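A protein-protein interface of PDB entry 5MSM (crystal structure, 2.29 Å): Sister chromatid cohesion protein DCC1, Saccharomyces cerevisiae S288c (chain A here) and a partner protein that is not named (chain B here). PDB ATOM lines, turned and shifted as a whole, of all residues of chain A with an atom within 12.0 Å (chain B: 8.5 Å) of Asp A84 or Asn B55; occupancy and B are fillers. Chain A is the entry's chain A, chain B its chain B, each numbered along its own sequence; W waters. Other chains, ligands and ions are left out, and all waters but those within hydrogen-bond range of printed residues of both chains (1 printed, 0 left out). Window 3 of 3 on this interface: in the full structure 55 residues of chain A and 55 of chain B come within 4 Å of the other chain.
The backbone NH (N) of Asp A84 sits at hydrogen-bond distance from the backbone carbonyl oxygen (O) of Asn B55 (2.7 Å).
The backbone carbonyl oxygen (O) of Glu B56 sits at hydrogen-bond distance from the guanidinium group (NH2) of Arg B69 (2.9 Å).
OE1 of Glu B56 lies within salt-bridge range of NZ of Lys B86.
The backbone carbonyl oxygen (O) of Gly B57 sits at hydrogen-bond distance from the guanidinium group (NE) of Arg B69, at 2.9 Å.
O of Arg B69 lies within hydrogen-bond range of NH1 of Arg B58, 2.5 Å away.
His A6 touches Arg B69.
CD of Arg B69 touches CG2 of Ile A81, at 3.8 Å.
Pro B54 touches Thr A82.
Gly B57 touches Thr A82.
Pro B54 touches Phe A83.
Asn B55 touches Phe A83 (O to CA, 3.5 Å).
Phe A83 touches Glu B56 (CB to O, 3.1 Å).
Phe A83 touches Gly B57.
Phe A83 touches Arg B69.
Of the printed residues of chain A, Asn B55 touches Phe A83 and Asp A84.
No residue of chain A comes within 4 Å of Ser B53.
Printed residues of chain A within 4 Å of Glu B56: Phe A83.
Printed residues of chain B within 4 Å of Thr A82: Pro B54 and Gly B57.
Printed residues of chain B within 4 Å of Ile A81: Arg B69 (3.8 Å).
Printed residues of chain B within 4 Å of Phe A83: Pro B54 (3.9 Å), Asn B55 (3.5 Å), Glu B56 (3.1 Å), Gly B57 (3.8 Å) and Arg B69 (3.5 Å).
Of the printed residues of chain B, His A6 touches Arg B69.
Ser A92 touches none of the printed residues of chain B.
The nearest printed residue of chain B that does not touch Ile A81 is Gly B57 (4.8 Å).
Of the 17 printed residues of chain A, 5 touch a printed residue of chain B.
Hydrophobic or aromatic side chains of chain A that line the printed part of chain B: His A6, Ile A81 and Phe A83.
Among the printed residues, 10 pairs touch across the chains.
Water W1 lies within hydrogen-bond range of the guanidinium group (NH1) of Arg B69 (2.6 Å) and the side-chain amide oxygen (OD1) of Asn A4 (2.8 Å).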
ATOM      1  N   SER A   2      31.361 -19.364  23.958  1.00  0.00           N
ATOM      2  CA  SER A   2      32.522 -19.055  23.138  1.00  0.00           C
ATOM      3  C   SER A   2      33.348 -17.963  23.778  1.00  0.00           C
ATOM      4  O   SER A   2      32.911 -17.296  24.710  1.00  0.00           O
ATOM      5  CB  SER A   2      32.122 -18.611  21.738  1.00  0.00           C
ATOM      6  OG  SER A   2      31.661 -17.272  21.760  1.00  0.00           O
ATOM      7  N   ASN A   4      35.452 -14.449  22.933  1.00  0.00           N
ATOM      8  CA  ASN A   4      35.785 -13.355  22.002  1.00  0.00           C
ATOM      9  C   ASN A   4      37.300 -13.136  21.933  1.00  0.00           C
ATOM     10  O   ASN A   4      37.969 -13.038  22.977  1.00  0.00           O
ATOM     11  CB  ASN A   4      35.125 -12.032  22.410  1.00  0.00           C
ATOM     12  CG  ASN A   4      33.597 -12.032  22.238  1.00  0.00           C
ATOM     13  OD1 ASN A   4      33.045 -12.735  21.390  1.00  0.00           O
ATOM     14  ND2 ASN A   4      32.919 -11.219  23.040  1.00  0.00           N
ATOM     15  N   HIS A   6      40.466 -10.786  20.715  1.00  0.00           N
ATOM     16  CA  HIS A   6      40.873  -9.442  20.371  1.00  0.00           C
ATOM     17  C   HIS A   6      42.384  -9.395  20.143  1.00  0.00           C
ATOM     18  O   HIS A   6      43.143 -10.239  20.642  1.00  0.00           O
ATOM     19  CB  HIS A   6      40.498  -8.454  21.473  1.00  0.00           C
ATOM     20  CG  HIS A   6      39.046  -8.429  21.800  1.00  0.00           C
ATOM     21  ND1 HIS A   6      38.166  -7.552  21.199  1.00  0.00           N
ATOM     22  CD2 HIS A   6      38.311  -9.170  22.663  1.00  0.00           C
ATOM     23  CE1 HIS A   6      36.956  -7.753  21.680  1.00  0.00           C
ATOM     24  NE2 HIS A   6      37.019  -8.722  22.578  1.00  0.00           N
ATOM     25  N   PRO A  80      30.758  -3.291  27.874  1.00  0.00           N
ATOM     26  CA  PRO A  80      30.459  -4.626  27.336  1.00  0.00           C
ATOM     27  C   PRO A  80      30.727  -4.697  25.833  1.00  0.00           C
ATOM     28  O   PRO A  80      30.503  -3.707  25.132  1.00  0.00           O
ATOM     29  CB  PRO A  80      28.963  -4.807  27.636  1.00  0.00           C
ATOM     30  CG  PRO A  80      28.695  -3.861  28.751  1.00  0.00           C
ATOM     31  CD  PRO A  80      29.557  -2.663  28.442  1.00  0.00           C
ATOM     32  N   ILE A  81      31.233  -5.832  25.360  1.00  0.00           N
ATOM     33  CA  ILE A  81      31.523  -6.005  23.942  1.00  0.00           C
ATOM     34  C   ILE A  81      30.248  -6.466  23.233  1.00  0.00           C
ATOM     35  O   ILE A  81      29.887  -7.645  23.298  1.00  0.00           O
ATOM     36  CB  ILE A  81      32.662  -7.028  23.720  1.00  0.00           C
ATOM     37  CG1 ILE A  81      33.960  -6.550  24.407  1.00  0.00           C
ATOM     38  CG2 ILE A  81      32.882  -7.296  22.231  1.00  0.00           C
ATOM     39  CD1 ILE A  81      34.574  -5.249  23.809  1.00  0.00           C
ATOM     40  N   THR A  82      29.586  -5.530  22.555  1.00  0.00           N
ATOM     41  CA  THR A  82      28.325  -5.816  21.867  1.00  0.00           C
ATOM     42  C   THR A  82      28.526  -5.721  20.359  1.00  0.00           C
ATOM     43  O   THR A  82      29.225  -4.823  19.874  1.00  0.00           O
ATOM     44  CB  THR A  82      27.189  -4.858  22.318  1.00  0.00           C
ATOM     45  OG1 THR A  82      27.575  -3.488  22.109  1.00  0.00           O
ATOM     46  CG2 THR A  82      26.919  -5.055  23.791  1.00  0.00           C
ATOM     47  N   PHE A  83      27.932  -6.672  19.643  1.00  0.00           N
ATOM     48  CA  PHE A  83      27.962  -6.737  18.184  1.00  0.00           C
ATOM     49  C   PHE A  83      26.835  -7.657  17.720  1.00  0.00           C
ATOM     50  O   PHE A  83      26.390  -8.504  18.482  1.00  0.00           O
ATOM     51  CB  PHE A  83      29.314  -7.272  17.691  1.00  0.00           C
ATOM     52  CG  PHE A  83      29.650  -8.644  18.212  1.00  0.00           C
ATOM     53  CD1 PHE A  83      30.332  -8.794  19.415  1.00  0.00           C
ATOM     54  CD2 PHE A  83      29.279  -9.796  17.502  1.00  0.00           C
ATOM     55  CE1 PHE A  83      30.651 -10.066  19.907  1.00  0.00           C
ATOM     56  CE2 PHE A  83      29.584 -11.062  17.981  1.00  0.00           C
ATOM     57  CZ  PHE A  83      30.281 -11.199  19.191  1.00  0.00           C
ATOM     58  N   ASP A  84      26.382  -7.515  16.482  1.00  0.00           N
ATOM     59  CA  ASP A  84      25.422  -8.472  15.955  1.00  0.00           C
ATOM     60  C   ASP A  84      26.105  -9.771  15.536  1.00  0.00           C
ATOM     61  O   ASP A  84      26.922  -9.769  14.613  1.00  0.00           O
ATOM     62  CB  ASP A  84      24.698  -7.886  14.736  1.00  0.00           C
ATOM     63  CG  ASP A  84      23.700  -6.806  15.095  1.00  0.00           C
ATOM     64  OD1 ASP A  84      23.503  -6.527  16.295  1.00  0.00           O
ATOM     65  OD2 ASP A  84      23.118  -6.219  14.157  1.00  0.00           O
ATOM     66  N   GLU A  85      25.743 -10.884  16.164  1.00  0.00           N
ATOM     67  CA  GLU A  85      26.112 -12.184  15.610  1.00  0.00           C
ATOM     68  C   GLU A  85      25.130 -12.526  14.475  1.00  0.00           C
ATOM     69  O   GLU A  85      23.912 -12.462  14.678  1.00  0.00           O
ATOM     70  CB  GLU A  85      26.128 -13.264  16.692  1.00  0.00           C
ATOM     71  CG  GLU A  85      26.670 -14.587  16.180  1.00  0.00           C
ATOM     72  CD  GLU A  85      27.938 -14.417  15.354  1.00  0.00           C
ATOM     73  OE1 GLU A  85      29.038 -14.436  15.947  1.00  0.00           O
ATOM     74  OE2 GLU A  85      27.837 -14.247  14.113  1.00  0.00           O
ATOM     75  N   THR A  86      25.632 -12.920  13.301  1.00  0.00           N
ATOM     76  CA  THR A  86      24.726 -13.136  12.169  1.00  0.00           C
ATOM     77  C   THR A  86      24.385 -14.581  11.831  1.00  0.00           C
ATOM     78  O   THR A  86      23.348 -14.851  11.230  1.00  0.00           O
ATOM     79  CB  THR A  86      25.312 -12.510  10.879  1.00  0.00           C
ATOM     80  OG1 THR A  86      24.271 -12.348   9.908  1.00  0.00           O
ATOM     81  CG2 THR A  86      26.420 -13.389  10.295  1.00  0.00           C
ATOM     82  N   LEU A  87      25.206 -15.519  12.269  1.00  0.00           N
ATOM     83  CA  LEU A  87      24.879 -16.913  12.045  1.00  0.00           C
ATOM     84  C   LEU A  87      24.669 -17.575  13.378  1.00  0.00           C
ATOM     85  O   LEU A  87      25.157 -17.106  14.411  1.00  0.00           O
ATOM     86  CB  LEU A  87      25.978 -17.648  11.276  1.00  0.00           C
ATOM     87  CG  LEU A  87      27.100 -18.260  12.115  1.00  0.00           C
ATOM     88  CD1 LEU A  87      27.699 -19.421  11.360  1.00  0.00           C
ATOM     89  CD2 LEU A  87      28.172 -17.247  12.449  1.00  0.00           C
ATOM     90  N   LEU A  88      23.908 -18.650  13.364  1.00  0.00           N
ATOM     91  CA  LEU A  88      23.924 -19.555  14.489  1.00  0.00           C
ATOM     92  C   LEU A  88      25.280 -20.250  14.633  1.00  0.00           C
ATOM     93  O   LEU A  88      26.023 -20.055  15.614  1.00  0.00           O
ATOM     94  CB  LEU A  88      22.828 -20.610  14.357  1.00  0.00           C
ATOM     95  CG  LEU A  88      22.250 -21.087  15.689  1.00  0.00           C
ATOM     96  CD1 LEU A  88      21.587 -19.931  16.441  1.00  0.00           C
ATOM     97  CD2 LEU A  88      21.276 -22.250  15.491  1.00  0.00           C
ATOM     98  N   PHE A  89      25.598 -21.034  13.609  1.00  0.00           N
ATOM     99  CA  PHE A  89      25.842 -22.437  13.847  1.00  0.00           C
ATOM    100  C   PHE A  89      27.210 -22.762  14.378  1.00  0.00           C
ATOM    101  O   PHE A  89      28.221 -22.288  13.880  1.00  0.00           O
ATOM    102  CB  PHE A  89      25.548 -23.184  12.548  1.00  0.00           C
ATOM    103  CG  PHE A  89      24.177 -22.877  12.014  1.00  0.00           C
ATOM    104  CD1 PHE A  89      23.053 -23.464  12.566  1.00  0.00           C
ATOM    105  CD2 PHE A  89      24.008 -21.965  10.976  1.00  0.00           C
ATOM    106  CE1 PHE A  89      21.789 -23.150  12.089  1.00  0.00           C
ATOM    107  CE2 PHE A  89      22.737 -21.651  10.487  1.00  0.00           C
ATOM    108  CZ  PHE A  89      21.636 -22.241  11.045  1.00  0.00           C
ATOM    109  N   LEU A  91      28.266 -21.840  17.394  1.00  0.00           N
ATOM    110  CA  LEU A  91      28.913 -20.743  18.097  1.00  0.00           C
ATOM    111  C   LEU A  91      28.023 -20.292  19.267  1.00  0.00           C
ATOM    112  O   LEU A  91      27.025 -19.611  19.058  1.00  0.00           O
ATOM    113  CB  LEU A  91      29.208 -19.610  17.102  1.00  0.00           C
ATOM    114  CG  LEU A  91      30.390 -18.652  17.355  1.00  0.00           C
ATOM    115  CD1 LEU A  91      30.432 -17.535  16.303  1.00  0.00           C
ATOM    116  CD2 LEU A  91      30.443 -18.075  18.748  1.00  0.00           C
ATOM    117  N   SER A  92      28.355 -20.704  20.489  1.00  0.00           N
ATOM    118  CA  SER A  92      27.611 -20.278  21.681  1.00  0.00           C
ATOM    119  C   SER A  92      27.865 -18.810  22.010  1.00  0.00           C
ATOM    120  O   SER A  92      28.758 -18.187  21.434  1.00  0.00           O
ATOM    121  CB  SER A  92      27.981 -21.147  22.873  1.00  0.00           C
ATOM    122  OG  SER A  92      29.381 -21.098  23.112  1.00  0.00           O
ATOM    123  N   LYS A  93      27.087 -18.250  22.930  1.00  0.00           N
ATOM    124  CA  LYS A  93      27.227 -16.842  23.318  1.00  0.00           C
ATOM    125  C   LYS A  93      28.591 -16.574  23.968  1.00  0.00           C
ATOM    126  O   LYS A  93      29.117 -17.442  24.653  1.00  0.00           O
ATOM    127  CB  LYS A  93      26.105 -16.454  24.279  1.00  0.00           C
ATOM    128  CG  LYS A  93      25.782 -14.971  24.287  1.00  0.00           C
ATOM    129  CD  LYS A  93      24.273 -14.733  24.319  1.00  0.00           C
ATOM    130  CE  LYS A  93      23.613 -15.134  22.991  1.00  0.00           C
ATOM    131  NZ  LYS A  93      22.113 -15.145  23.045  1.00  0.00           N
ATOM    132  N   PRO A  94      29.174 -15.379  23.750  1.00  0.00           N
ATOM    133  CA  PRO A  94      30.477 -15.101  24.372  1.00  0.00           C
ATOM    134  C   PRO A  94      30.378 -15.136  25.886  1.00  0.00           C
ATOM    135  O   PRO A  94      29.422 -14.573  26.410  1.00  0.00           O
ATOM    136  CB  PRO A  94      30.818 -13.673  23.917  1.00  0.00           C
ATOM    137  CG  PRO A  94      29.811 -13.290  22.928  1.00  0.00           C
ATOM    138  CD  PRO A  94      28.800 -14.367  22.749  1.00  0.00           C
ATOM    139  N   ASP B  52      33.385   2.632  12.788  1.00  0.00           N
ATOM    140  CA  ASP B  52      32.930   1.347  13.307  1.00  0.00           C
ATOM    141  C   ASP B  52      31.508   1.424  13.818  1.00  0.00           C
ATOM    142  O   ASP B  52      31.194   2.225  14.694  1.00  0.00           O
ATOM    143  CB  ASP B  52      33.876   0.866  14.425  1.00  0.00           C
ATOM    144  CG  ASP B  52      33.467  -0.468  15.019  1.00  0.00           C
ATOM    145  OD1 ASP B  52      33.135  -1.393  14.243  1.00  0.00           O
ATOM    146  OD2 ASP B  52      33.518  -0.601  16.264  1.00  0.00           O
ATOM    147  N   SER B  53      30.647   0.610  13.221  1.00  0.00           N
ATOM    148  CA  SER B  53      29.255   0.496  13.636  1.00  0.00           C
ATOM    149  C   SER B  53      29.157  -0.216  14.982  1.00  0.00           C
ATOM    150  O   SER B  53      30.082  -0.927  15.376  1.00  0.00           O
ATOM    151  CB  SER B  53      28.466  -0.289  12.593  1.00  0.00           C
ATOM    152  OG  SER B  53      29.033  -0.120  11.306  1.00  0.00           O
ATOM    153  N   PRO B  54      28.025  -0.052  15.695  1.00  0.00           N
ATOM    154  CA  PRO B  54      27.937  -0.814  16.945  1.00  0.00           C
ATOM    155  C   PRO B  54      27.284  -2.146  16.643  1.00  0.00           C
ATOM    156  O   PRO B  54      27.129  -2.989  17.521  1.00  0.00           O
ATOM    157  CB  PRO B  54      27.032   0.047  17.828  1.00  0.00           C
ATOM    158  CG  PRO B  54      26.131   0.730  16.851  1.00  0.00           C
ATOM    159  CD  PRO B  54      26.893   0.879  15.537  1.00  0.00           C
ATOM    160  N   ASN B  55      26.912  -2.319  15.380  1.00  0.00           N
ATOM    161  CA  ASN B  55      26.483  -3.602  14.854  1.00  0.00           C
ATOM    162  C   ASN B  55      27.668  -4.511  14.567  1.00  0.00           C
ATOM    163  O   ASN B  55      27.631  -5.710  14.845  1.00  0.00           O
ATOM    164  CB  ASN B  55      25.636  -3.401  13.602  1.00  0.00           C
ATOM    165  CG  ASN B  55      24.192  -3.085  13.933  1.00  0.00           C
ATOM    166  OD1 ASN B  55      23.838  -2.855  15.103  1.00  0.00           O
ATOM    167  ND2 ASN B  55      23.342  -3.065  12.903  1.00  0.00           N
ATOM    168  N   GLU B  56      28.727  -3.943  14.009  1.00  0.00           N
ATOM    169  CA  GLU B  56      29.924  -4.733  13.814  1.00  0.00           C
ATOM    170  C   GLU B  56      30.654  -4.973  15.135  1.00  0.00           C
ATOM    171  O   GLU B  56      31.070  -6.096  15.405  1.00  0.00           O
ATOM    172  CB  GLU B  56      30.847  -4.044  12.815  1.00  0.00           C
ATOM    173  CG  GLU B  56      30.170  -3.659  11.532  1.00  0.00           C
ATOM    174  CD  GLU B  56      29.922  -4.874  10.676  1.00  0.00           C
ATOM    175  OE1 GLU B  56      30.676  -5.860  10.836  1.00  0.00           O
ATOM    176  OE2 GLU B  56      28.972  -4.858   9.858  1.00  0.00           O
ATOM    177  N   GLY B  57      30.775  -3.946  15.969  1.00  0.00           N
ATOM    178  CA  GLY B  57      31.421  -4.117  17.255  1.00  0.00           C
ATOM    179  C   GLY B  57      32.847  -4.609  17.071  1.00  0.00           C
ATOM    180  O   GLY B  57      33.277  -5.535  17.759  1.00  0.00           O
ATOM    181  N   ARG B  58      33.564  -4.041  16.105  1.00  0.00           N
ATOM    182  CA  ARG B  58      34.895  -4.559  15.778  1.00  0.00           C
ATOM    183  C   ARG B  58      36.047  -3.906  16.553  1.00  0.00           C
ATOM    184  O   ARG B  58      37.145  -4.452  16.607  1.00  0.00           O
ATOM    185  CB  ARG B  58      35.154  -4.438  14.283  1.00  0.00           C
ATOM    186  CG  ARG B  58      34.458  -5.504  13.450  1.00  0.00           C
ATOM    187  CD  ARG B  58      34.999  -6.887  13.738  1.00  0.00           C
ATOM    188  NE  ARG B  58      34.226  -7.912  13.058  1.00  0.00           N
ATOM    189  CZ  ARG B  58      34.355  -9.218  13.269  1.00  0.00           C
ATOM    190  NH1 ARG B  58      35.244  -9.651  14.137  1.00  0.00           N
ATOM    191  NH2 ARG B  58      33.599 -10.092  12.611  1.00  0.00           N
ATOM    192  N   ARG B  69      38.385  -6.750  17.420  1.00  0.00           N
ATOM    193  CA  ARG B  69      37.771  -8.027  17.726  1.00  0.00           C
ATOM    194  C   ARG B  69      37.840  -8.860  16.468  1.00  0.00           C
ATOM    195  O   ARG B  69      37.081  -8.614  15.523  1.00  0.00           O
ATOM    196  CB  ARG B  69      36.307  -7.834  18.184  1.00  0.00           C
ATOM    197  CG  ARG B  69      35.591  -9.115  18.640  1.00  0.00           C
ATOM    198  CD  ARG B  69      34.105  -8.873  18.979  1.00  0.00           C
ATOM    199  NE  ARG B  69      33.360  -8.403  17.805  1.00  0.00           N
ATOM    200  CZ  ARG B  69      32.876  -9.219  16.877  1.00  0.00           C
ATOM    201  NH1 ARG B  69      33.083 -10.523  16.979  1.00  0.00           N
ATOM    202  NH2 ARG B  69      32.222  -8.734  15.833  1.00  0.00           N
ATOM    203  N   LYS B  86      34.174 -12.301   9.159  1.00  0.00           N
ATOM    204  CA  LYS B  86      32.793 -12.633   8.852  1.00  0.00           C
ATOM    205  C   LYS B  86      32.679 -13.929   8.076  1.00  0.00           C
ATOM    206  O   LYS B  86      31.625 -14.560   8.064  1.00  0.00           O
ATOM    207  CB  LYS B  86      32.136 -11.503   8.059  1.00  0.00           C
ATOM    208  CG  LYS B  86      32.746 -10.138   8.322  1.00  0.00           C
ATOM    209  CD  LYS B  86      31.854  -9.005   7.799  1.00  0.00           C
ATOM    210  CE  LYS B  86      32.527  -7.637   7.997  1.00  0.00           C
ATOM    211  NZ  LYS B  86      31.808  -6.521   7.301  1.00  0.00           N
HETATM  212  O   HOH W   1      34.000 -12.053  18.808  1.00  0.00           O
